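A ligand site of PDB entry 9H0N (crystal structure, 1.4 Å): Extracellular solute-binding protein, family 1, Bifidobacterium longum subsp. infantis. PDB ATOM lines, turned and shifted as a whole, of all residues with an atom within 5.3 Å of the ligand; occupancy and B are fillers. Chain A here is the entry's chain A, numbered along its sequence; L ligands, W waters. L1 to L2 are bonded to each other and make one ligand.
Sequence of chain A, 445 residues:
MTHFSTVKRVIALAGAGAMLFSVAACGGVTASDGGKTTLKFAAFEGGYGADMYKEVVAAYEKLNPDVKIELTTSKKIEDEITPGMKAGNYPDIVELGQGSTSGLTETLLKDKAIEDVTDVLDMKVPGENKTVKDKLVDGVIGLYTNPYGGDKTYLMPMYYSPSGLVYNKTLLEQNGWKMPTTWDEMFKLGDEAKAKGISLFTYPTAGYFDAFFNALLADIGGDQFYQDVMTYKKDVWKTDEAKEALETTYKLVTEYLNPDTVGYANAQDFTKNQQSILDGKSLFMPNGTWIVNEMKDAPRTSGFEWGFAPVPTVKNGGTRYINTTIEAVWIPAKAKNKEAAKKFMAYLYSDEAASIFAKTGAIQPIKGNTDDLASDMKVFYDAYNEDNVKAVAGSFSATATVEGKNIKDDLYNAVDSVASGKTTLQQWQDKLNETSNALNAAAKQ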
ATOM      1  N   PHE A  44      23.009  -2.254   4.382  1.00  0.00           N
ATOM      2  CA  PHE A  44      23.301  -2.085   5.801  1.00  0.00           C
ATOM      3  C   PHE A  44      22.238  -1.225   6.489  1.00  0.00           C
ATOM      4  O   PHE A  44      21.915  -0.118   6.041  1.00  0.00           O
ATOM      5  CB  PHE A  44      24.667  -1.433   5.969  1.00  0.00           C
ATOM      6  CG  PHE A  44      25.072  -1.248   7.417  1.00  0.00           C
ATOM      7  CD1 PHE A  44      25.442  -2.328   8.192  1.00  0.00           C
ATOM      8  CD2 PHE A  44      25.072   0.024   7.997  1.00  0.00           C
ATOM      9  CE1 PHE A  44      25.809  -2.156   9.538  1.00  0.00           C
ATOM     10  CE2 PHE A  44      25.440   0.192   9.329  1.00  0.00           C
ATOM     11  CZ  PHE A  44      25.803  -0.900  10.099  1.00  0.00           C
ATOM     12  N   GLY A  46      21.781   1.102   9.199  1.00  0.00           N
ATOM     13  CA  GLY A  46      22.486   2.011  10.060  1.00  0.00           C
ATOM     14  C   GLY A  46      21.561   3.008  10.697  1.00  0.00           C
ATOM     15  O   GLY A  46      20.329   2.821  10.732  1.00  0.00           O
ATOM     16  N   GLY A  47      22.140   4.104  11.177  1.00  0.00           N
ATOM     17  CA  GLY A  47      21.401   5.075  11.977  1.00  0.00           C
ATOM     18  C   GLY A  47      20.308   5.811  11.221  1.00  0.00           C
ATOM     19  O   GLY A  47      19.396   6.357  11.870  1.00  0.00           O
ATOM     20  N   TYR A  48      20.368   5.839   9.894  1.00  0.00           N
ATOM     21  CA  TYR A  48      19.299   6.437   9.095  1.00  0.00           C
ATOM     22  C   TYR A  48      18.114   5.503   8.920  1.00  0.00           C
ATOM     23  O   TYR A  48      17.071   5.943   8.412  1.00  0.00           O
ATOM     24  CB  TYR A  48      19.821   6.864   7.711  1.00  0.00           C
ATOM     25  CG  TYR A  48      20.929   7.900   7.692  1.00  0.00           C
ATOM     26  CD1 TYR A  48      20.713   9.190   8.181  1.00  0.00           C
ATOM     27  CD2 TYR A  48      22.171   7.602   7.121  1.00  0.00           C
ATOM     28  CE1 TYR A  48      21.734  10.149   8.130  1.00  0.00           C
ATOM     29  CE2 TYR A  48      23.178   8.541   7.073  1.00  0.00           C
ATOM     30  CZ  TYR A  48      22.952   9.806   7.575  1.00  0.00           C
ATOM     31  OH  TYR A  48      23.972  10.738   7.487  1.00  0.00           O
ATOM     32  N   GLN A  98      33.027   1.446   3.510  1.00  0.00           N
ATOM     33  CA  GLN A  98      34.272   1.150   4.198  1.00  0.00           C
ATOM     34  C   GLN A  98      34.102   1.469   5.676  1.00  0.00           C
ATOM     35  O   GLN A  98      33.262   2.280   6.067  1.00  0.00           O
ATOM     36  CB  GLN A  98      35.399   2.020   3.659  1.00  0.00           C
ATOM     37  CG  GLN A  98      35.669   1.849   2.167  1.00  0.00           C
ATOM     38  CD  GLN A  98      37.074   2.315   1.778  1.00  0.00           C
ATOM     39  OE1 GLN A  98      38.039   2.043   2.485  1.00  0.00           O
ATOM     40  NE2 GLN A  98      37.193   3.042   0.669  1.00  0.00           N
ATOM     41  N   GLY A  99      34.908   0.828   6.513  1.00  0.00           N
ATOM     42  CA  GLY A  99      34.840   1.110   7.936  1.00  0.00           C
ATOM     43  C   GLY A  99      33.773   0.363   8.699  1.00  0.00           C
ATOM     44  O   GLY A  99      33.632   0.579   9.920  1.00  0.00           O
ATOM     45  N   SER A 100      33.014  -0.515   8.052  1.00  0.00           N
ATOM     46  CA  SER A 100      31.951  -1.195   8.768  1.00  0.00           C
ATOM     47  C   SER A 100      32.532  -2.206   9.751  1.00  0.00           C
ATOM     48  O   SER A 100      33.708  -2.589   9.693  1.00  0.00           O
ATOM     49  CB  SER A 100      31.019  -1.900   7.791  1.00  0.00           C
ATOM     50  OG  SER A 100      31.599  -3.102   7.356  1.00  0.00           O
ATOM     51  N   THR A 101      31.662  -2.640  10.680  1.00  0.00           N
ATOM     52  CA  THR A 101      32.072  -3.576  11.730  1.00  0.00           C
ATOM     53  C   THR A 101      32.856  -4.752  11.169  1.00  0.00           C
ATOM     54  O   THR A 101      33.942  -5.086  11.655  1.00  0.00           O
ATOM     55  CB  THR A 101      30.831  -4.088  12.461  1.00  0.00           C
ATOM     56  OG1 THR A 101      30.087  -2.981  12.999  1.00  0.00           O
ATOM     57  CG2 THR A 101      31.222  -5.026  13.583  1.00  0.00           C
ATOM     58  N   TYR A 159      25.110   8.824   0.716  1.00  0.00           N
ATOM     59  CA  TYR A 159      24.997   9.807   1.805  1.00  0.00           C
ATOM     60  C   TYR A 159      25.995  10.945   1.611  1.00  0.00           C
ATOM     61  O   TYR A 159      26.706  11.004   0.601  1.00  0.00           O
ATOM     62  CB  TYR A 159      25.152   9.156   3.192  1.00  0.00           C
ATOM     63  CG  TYR A 159      24.369   7.866   3.452  1.00  0.00           C
ATOM     64  CD1 TYR A 159      23.173   7.573   2.799  1.00  0.00           C
ATOM     65  CD2 TYR A 159      24.852   6.935   4.361  1.00  0.00           C
ATOM     66  CE1 TYR A 159      22.477   6.386   3.070  1.00  0.00           C
ATOM     67  CE2 TYR A 159      24.159   5.767   4.642  1.00  0.00           C
ATOM     68  CZ  TYR A 159      22.990   5.488   3.967  1.00  0.00           C
ATOM     69  OH  TYR A 159      22.319   4.318   4.265  1.00  0.00           O
ATOM     70  N   SER A 163      31.068  15.063   9.385  1.00  0.00           N
ATOM     71  CA  SER A 163      31.442  14.456  10.664  1.00  0.00           C
ATOM     72  C   SER A 163      32.400  15.377  11.392  1.00  0.00           C
ATOM     73  O   SER A 163      33.185  16.105  10.776  1.00  0.00           O
ATOM     74  CB  SER A 163      32.103  13.091  10.505  1.00  0.00           C
ATOM     75  OG  SER A 163      31.179  12.072  10.156  1.00  0.00           O
ATOM     76  N   THR A 205      32.325   3.502  18.624  1.00  0.00           N
ATOM     77  CA  THR A 205      33.338   2.465  18.489  1.00  0.00           C
ATOM     78  C   THR A 205      34.608   3.121  17.966  1.00  0.00           C
ATOM     79  O   THR A 205      34.603   4.242  17.463  1.00  0.00           O
ATOM     80  CB  THR A 205      32.974   1.356  17.490  1.00  0.00           C
ATOM     81  OG1 THR A 205      33.151   1.859  16.157  1.00  0.00           O
ATOM     82  CG2 THR A 205      31.544   0.843  17.698  1.00  0.00           C
ATOM     83  N   GLY A 207      36.116   2.571  15.331  1.00  0.00           N
ATOM     84  CA  GLY A 207      36.087   2.836  13.907  1.00  0.00           C
ATOM     85  C   GLY A 207      35.709   4.262  13.571  1.00  0.00           C
ATOM     86  O   GLY A 207      36.016   4.746  12.474  1.00  0.00           O
ATOM     87  N   TYR A 208      35.024   4.948  14.484  1.00  0.00           N
ATOM     88  CA  TYR A 208      34.653   6.335  14.275  1.00  0.00           C
ATOM     89  C   TYR A 208      35.850   7.260  14.293  1.00  0.00           C
ATOM     90  O   TYR A 208      35.715   8.438  13.954  1.00  0.00           O
ATOM     91  CB  TYR A 208      33.637   6.777  15.344  1.00  0.00           C
ATOM     92  CG  TYR A 208      32.249   6.204  15.176  1.00  0.00           C
ATOM     93  CD1 TYR A 208      31.999   4.852  15.361  1.00  0.00           C
ATOM     94  CD2 TYR A 208      31.178   7.031  14.868  1.00  0.00           C
ATOM     95  CE1 TYR A 208      30.715   4.317  15.201  1.00  0.00           C
ATOM     96  CE2 TYR A 208      29.875   6.513  14.709  1.00  0.00           C
ATOM     97  CZ  TYR A 208      29.665   5.144  14.888  1.00  0.00           C
ATOM     98  OH  TYR A 208      28.417   4.573  14.769  1.00  0.00           O
ATOM     99  N   ASP A 210      37.899   7.085  12.031  1.00  0.00           N
ATOM    100  CA  ASP A 210      38.173   7.353  10.620  1.00  0.00           C
ATOM    101  C   ASP A 210      37.991   8.827  10.275  1.00  0.00           C
ATOM    102  O   ASP A 210      38.911   9.492   9.768  1.00  0.00           O
ATOM    103  CB  ASP A 210      37.404   6.387   9.686  1.00  0.00           C
ATOM    104  CG  ASP A 210      35.884   6.402   9.848  1.00  0.00           C
ATOM    105  OD1 ASP A 210      35.301   7.178  10.623  1.00  0.00           O
ATOM    106  OD2 ASP A 210      35.249   5.589   9.137  1.00  0.00           O
ATOM    107  N   ALA A 211      36.814   9.377  10.583  1.00  0.00           N
ATOM    108  CA  ALA A 211      36.550  10.790  10.283  1.00  0.00           C
ATOM    109  C   ALA A 211      37.360  11.707  11.182  1.00  0.00           C
ATOM    110  O   ALA A 211      37.793  12.792  10.744  1.00  0.00           O
ATOM    111  CB  ALA A 211      35.048  11.076  10.423  1.00  0.00           C
ATOM    112  N   ALA A 267      29.822  -3.445  18.494  1.00  0.00           N
ATOM    113  CA  ALA A 267      28.611  -3.366  17.696  1.00  0.00           C
ATOM    114  C   ALA A 267      27.339  -3.538  18.521  1.00  0.00           C
ATOM    115  O   ALA A 267      26.267  -3.105  18.085  1.00  0.00           O
ATOM    116  CB  ALA A 267      28.654  -4.416  16.588  1.00  0.00           C
ATOM    117  N   PHE A 270      27.502   0.193  21.265  1.00  0.00           N
ATOM    118  CA  PHE A 270      27.963   1.526  20.905  1.00  0.00           C
ATOM    119  C   PHE A 270      26.947   2.602  21.235  1.00  0.00           C
ATOM    120  O   PHE A 270      27.334   3.741  21.541  1.00  0.00           O
ATOM    121  CB  PHE A 270      28.428   1.619  19.439  1.00  0.00           C
ATOM    122  CG  PHE A 270      27.300   1.595  18.440  1.00  0.00           C
ATOM    123  CD1 PHE A 270      26.693   0.387  18.102  1.00  0.00           C
ATOM    124  CD2 PHE A 270      26.886   2.760  17.800  1.00  0.00           C
ATOM    125  CE1 PHE A 270      25.675   0.337  17.156  1.00  0.00           C
ATOM    126  CE2 PHE A 270      25.851   2.723  16.842  1.00  0.00           C
ATOM    127  CZ  PHE A 270      25.250   1.501  16.530  1.00  0.00           C
ATOM    128  N   TRP A 290      23.630  10.982  11.054  1.00  0.00           N
ATOM    129  CA  TRP A 290      22.723   9.888  11.377  1.00  0.00           C
ATOM    130  C   TRP A 290      22.445   9.817  12.870  1.00  0.00           C
ATOM    131  O   TRP A 290      21.536   9.095  13.275  1.00  0.00           O
ATOM    132  CB  TRP A 290      23.282   8.527  10.886  1.00  0.00           C
ATOM    133  CG  TRP A 290      24.643   8.287  11.462  1.00  0.00           C
ATOM    134  CD1 TRP A 290      24.922   7.751  12.684  1.00  0.00           C
ATOM    135  CD2 TRP A 290      25.880   8.656  10.876  1.00  0.00           C
ATOM    136  NE1 TRP A 290      26.281   7.743  12.886  1.00  0.00           N
ATOM    137  CE2 TRP A 290      26.900   8.311  11.797  1.00  0.00           C
ATOM    138  CE3 TRP A 290      26.251   9.242   9.657  1.00  0.00           C
ATOM    139  CZ2 TRP A 290      28.259   8.522  11.526  1.00  0.00           C
ATOM    140  CZ3 TRP A 290      27.598   9.458   9.391  1.00  0.00           C
ATOM    141  CH2 TRP A 290      28.592   9.096  10.321  1.00  0.00           C
ATOM    142  N   GLU A 294      19.204   8.129  14.803  1.00  0.00           N
ATOM    143  CA  GLU A 294      19.577   6.909  15.526  1.00  0.00           C
ATOM    144  C   GLU A 294      19.165   6.978  16.985  1.00  0.00           C
ATOM    145  O   GLU A 294      18.790   5.965  17.586  1.00  0.00           O
ATOM    146  CB  GLU A 294      21.083   6.720  15.413  1.00  0.00           C
ATOM    147  CG  GLU A 294      21.593   5.372  15.888  1.00  0.00           C
ATOM    148  CD  GLU A 294      23.017   5.137  15.435  1.00  0.00           C
ATOM    149  OE1 GLU A 294      23.925   5.857  15.895  1.00  0.00           O
ATOM    150  OE2 GLU A 294      23.237   4.241  14.576  1.00  0.00           O
ATOM    151  N   THR A 325      31.577  12.517   5.220  1.00  0.00           N
ATOM    152  CA  THR A 325      31.517  11.071   5.381  1.00  0.00           C
ATOM    153  C   THR A 325      30.493  10.511   4.409  1.00  0.00           C
ATOM    154  O   THR A 325      29.338  10.947   4.375  1.00  0.00           O
ATOM    155  CB  THR A 325      31.079  10.730   6.802  1.00  0.00           C
ATOM    156  OG1 THR A 325      32.114  11.133   7.712  1.00  0.00           O
ATOM    157  CG2 THR A 325      30.854   9.240   6.967  1.00  0.00           C
ATOM    158  N   GLU A 327      29.079   6.614   2.697  1.00  0.00           N
ATOM    159  CA  GLU A 327      29.117   5.164   2.648  1.00  0.00           C
ATOM    160  C   GLU A 327      29.227   4.751   1.181  1.00  0.00           C
ATOM    161  O   GLU A 327      29.646   5.546   0.339  1.00  0.00           O
ATOM    162  CB  GLU A 327      27.928   4.551   3.395  1.00  0.00           C
ATOM    163  CG  GLU A 327      28.017   4.822   4.880  1.00  0.00           C
ATOM    164  CD  GLU A 327      26.924   4.139   5.683  1.00  0.00           C
ATOM    165  OE1 GLU A 327      26.247   3.197   5.191  1.00  0.00           O
ATOM    166  OE2 GLU A 327      26.757   4.572   6.839  1.00  0.00           O
HETATM  167  O1  LIG L   1      24.956   3.813  11.124  1.00  0.00           O
HETATM  168  C1  LIG L   1      25.493   3.280  12.312  1.00  0.00           C
HETATM  169  O2  LIG L   1      25.574   4.287  13.288  1.00  0.00           O
HETATM  170  C2  LIG L   1      26.884   2.661  12.092  1.00  0.00           C
HETATM  171  N1  LIG L   1      27.507   2.262  13.341  1.00  0.00           N
HETATM  172  C3  LIG L   1      27.825   3.635  11.385  1.00  0.00           C
HETATM  173  O3  LIG L   1      28.970   2.925  11.011  1.00  0.00           O
HETATM  174  C4  LIG L   1      27.149   4.187  10.136  1.00  0.00           C
HETATM  175  O4  LIG L   1      27.046   3.132   9.221  1.00  0.00           O
HETATM  176  C5  LIG L   1      25.781   4.782  10.488  1.00  0.00           C
HETATM  177  C6  LIG L   1      24.965   5.414   9.360  1.00  0.00           C
HETATM  178  O5  LIG L   1      24.598   4.445   8.413  1.00  0.00           O
HETATM  179  C7  LIG L   1      27.807   0.971  13.629  1.00  0.00           C
HETATM  180  O6  LIG L   1      27.533   0.043  12.878  1.00  0.00           O
HETATM  181  C8  LIG L   1      28.477   0.722  14.947  1.00  0.00           C
HETATM  182  C1  LG2 L   2      30.168   3.497  11.557  1.00  0.00           C
HETATM  183  C2  LG2 L   2      31.297   2.470  11.481  1.00  0.00           C
HETATM  184  C3  LG2 L   2      32.562   3.193  11.988  1.00  0.00           C
HETATM  185  C4  LG2 L   2      32.848   4.467  11.210  1.00  0.00           C
HETATM  186  C5  LG2 L   2      31.616   5.353  11.304  1.00  0.00           C
HETATM  187  C6  LG2 L   2      31.723   6.640  10.529  1.00  0.00           C
HETATM  188  O1  LG2 L   2      30.971   1.344  12.277  1.00  0.00           O
HETATM  189  O2  LG2 L   2      33.621   2.281  11.965  1.00  0.00           O
HETATM  190  O3  LG2 L   2      33.107   4.143   9.859  1.00  0.00           O
HETATM  191  O4  LG2 L   2      30.501   4.634  10.789  1.00  0.00           O
HETATM  192  O5  LG2 L   2      32.640   7.502  11.166  1.00  0.00           O
HETATM  193  O   HOH W   1      29.046   1.314   8.444  1.00  0.00           O
HETATM  194  O   HOH W   2      34.948  -0.683  13.047  1.00  0.00           O
HETATM  195  O   HOH W   3      31.615  10.000  12.008  1.00  0.00           O
HETATM  196  O   HOH W   4      25.359  -1.664  13.677  1.00  0.00           O
HETATM  197  O   HOH W   5      29.357  -0.342  10.706  1.00  0.00           O
HETATM  198  O   HOH W   6      32.676   0.125  14.068  1.00  0.00           O
HETATM  199  O   HOH W   7      23.533   2.555   5.788  1.00  0.00           O
HETATM  200  O   HOH W   8      26.543   6.265  15.369  1.00  0.00           O
HETATM  201  O   HOH W   9      21.846   4.308   7.936  1.00  0.00           O
HETATM  202  O   HOH W  10      31.365   2.941   8.008  1.00  0.00           O
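An oxygen (O3) of LG2 L2 is in hydrogen-bond range of the side-chain carboxylate (OD2) of Asp 210 (2.7 Å). OE2 of Glu 294 is in hydrogen-bond range of O2 of LIG L1 (2.7 Å). OE2 of Glu 327 lies within hydrogen-bond range of O5 of LIG L1, at 2.7 Å. An oxygen (O1) of LIG L1 sits at hydrogen-bond distance from the backbone NH (N) of Gly 47 (2.8 Å). O2 of LG2 L2 lies close to O of Gly 207, at 3.5 Å. An oxygen (O2) of LG2 L2 sits at hydrogen-bond distance from the backbone carbonyl oxygen (O) of Gly 99 (2.7 Å). N1 of LIG L1 sits at hydrogen-bond distance from OH of Tyr 208.
N of Glu 294 lies within hydrogen-bond range of O of Gly 47 (3.4 Å). OG1 of Thr 205 sits close to N of Gly 207, at 3.2 Å.
Merely in contact with the ligand: Phe 44 (3.4 Å), Gly 46 (3.2 Å), Thr 101 (3.96 Å), Phe 270 (3.6 Å) and Trp 290 (3.6 Å). Hydrophobic or aromatic side chains within 4 Å of the ligand: Phe 44, Tyr 208, Phe 270 and Trp 290. Of the 21 residues printed, 12 come within 4 Å of the ligand.
Water W6 lies within hydrogen-bond range of the side-chain hydroxyl (OG1) of Thr 205 (2.8 Å) and an oxygen (O1) of LG2 L2 (2.8 Å). Water W10 lies within hydrogen-bond range of the backbone carbonyl oxygen (O) of Gln 98 (2.8 Å) and an oxygen (O3) of LG2 L2 (2.8 Å). Water W5 bridges an oxygen (O1) of LG2 L2 (2.8 Å) and the backbone NH (N) of Thr 101 (3.3 Å). Water W3 bridges OG of Ser 163 (2.8 Å) and O5 of LG2 L2 (2.8 Å). Water W8 lies within hydrogen-bond range of the side-chain hydroxyl (OH) of Tyr 208 (2.6 Å), the side-chain carboxylate (OE1) of Glu 294 (2.7 Å), the indole nitrogen (NE1) of Trp 290 (2.9 Å) and an oxygen (O2) of LIG L1 (3.0 Å). Water W7 lies within hydrogen-bond range of the side-chain hydroxyl (OH) of Tyr 159 (2.6 Å), the side-chain carboxylate (OE1) of Glu 327 (2.9 Å), the backbone carbonyl oxygen (O) of Phe 44 (3.1 Å) and an oxygen (O5) of LIG L1 (3.4 Å).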
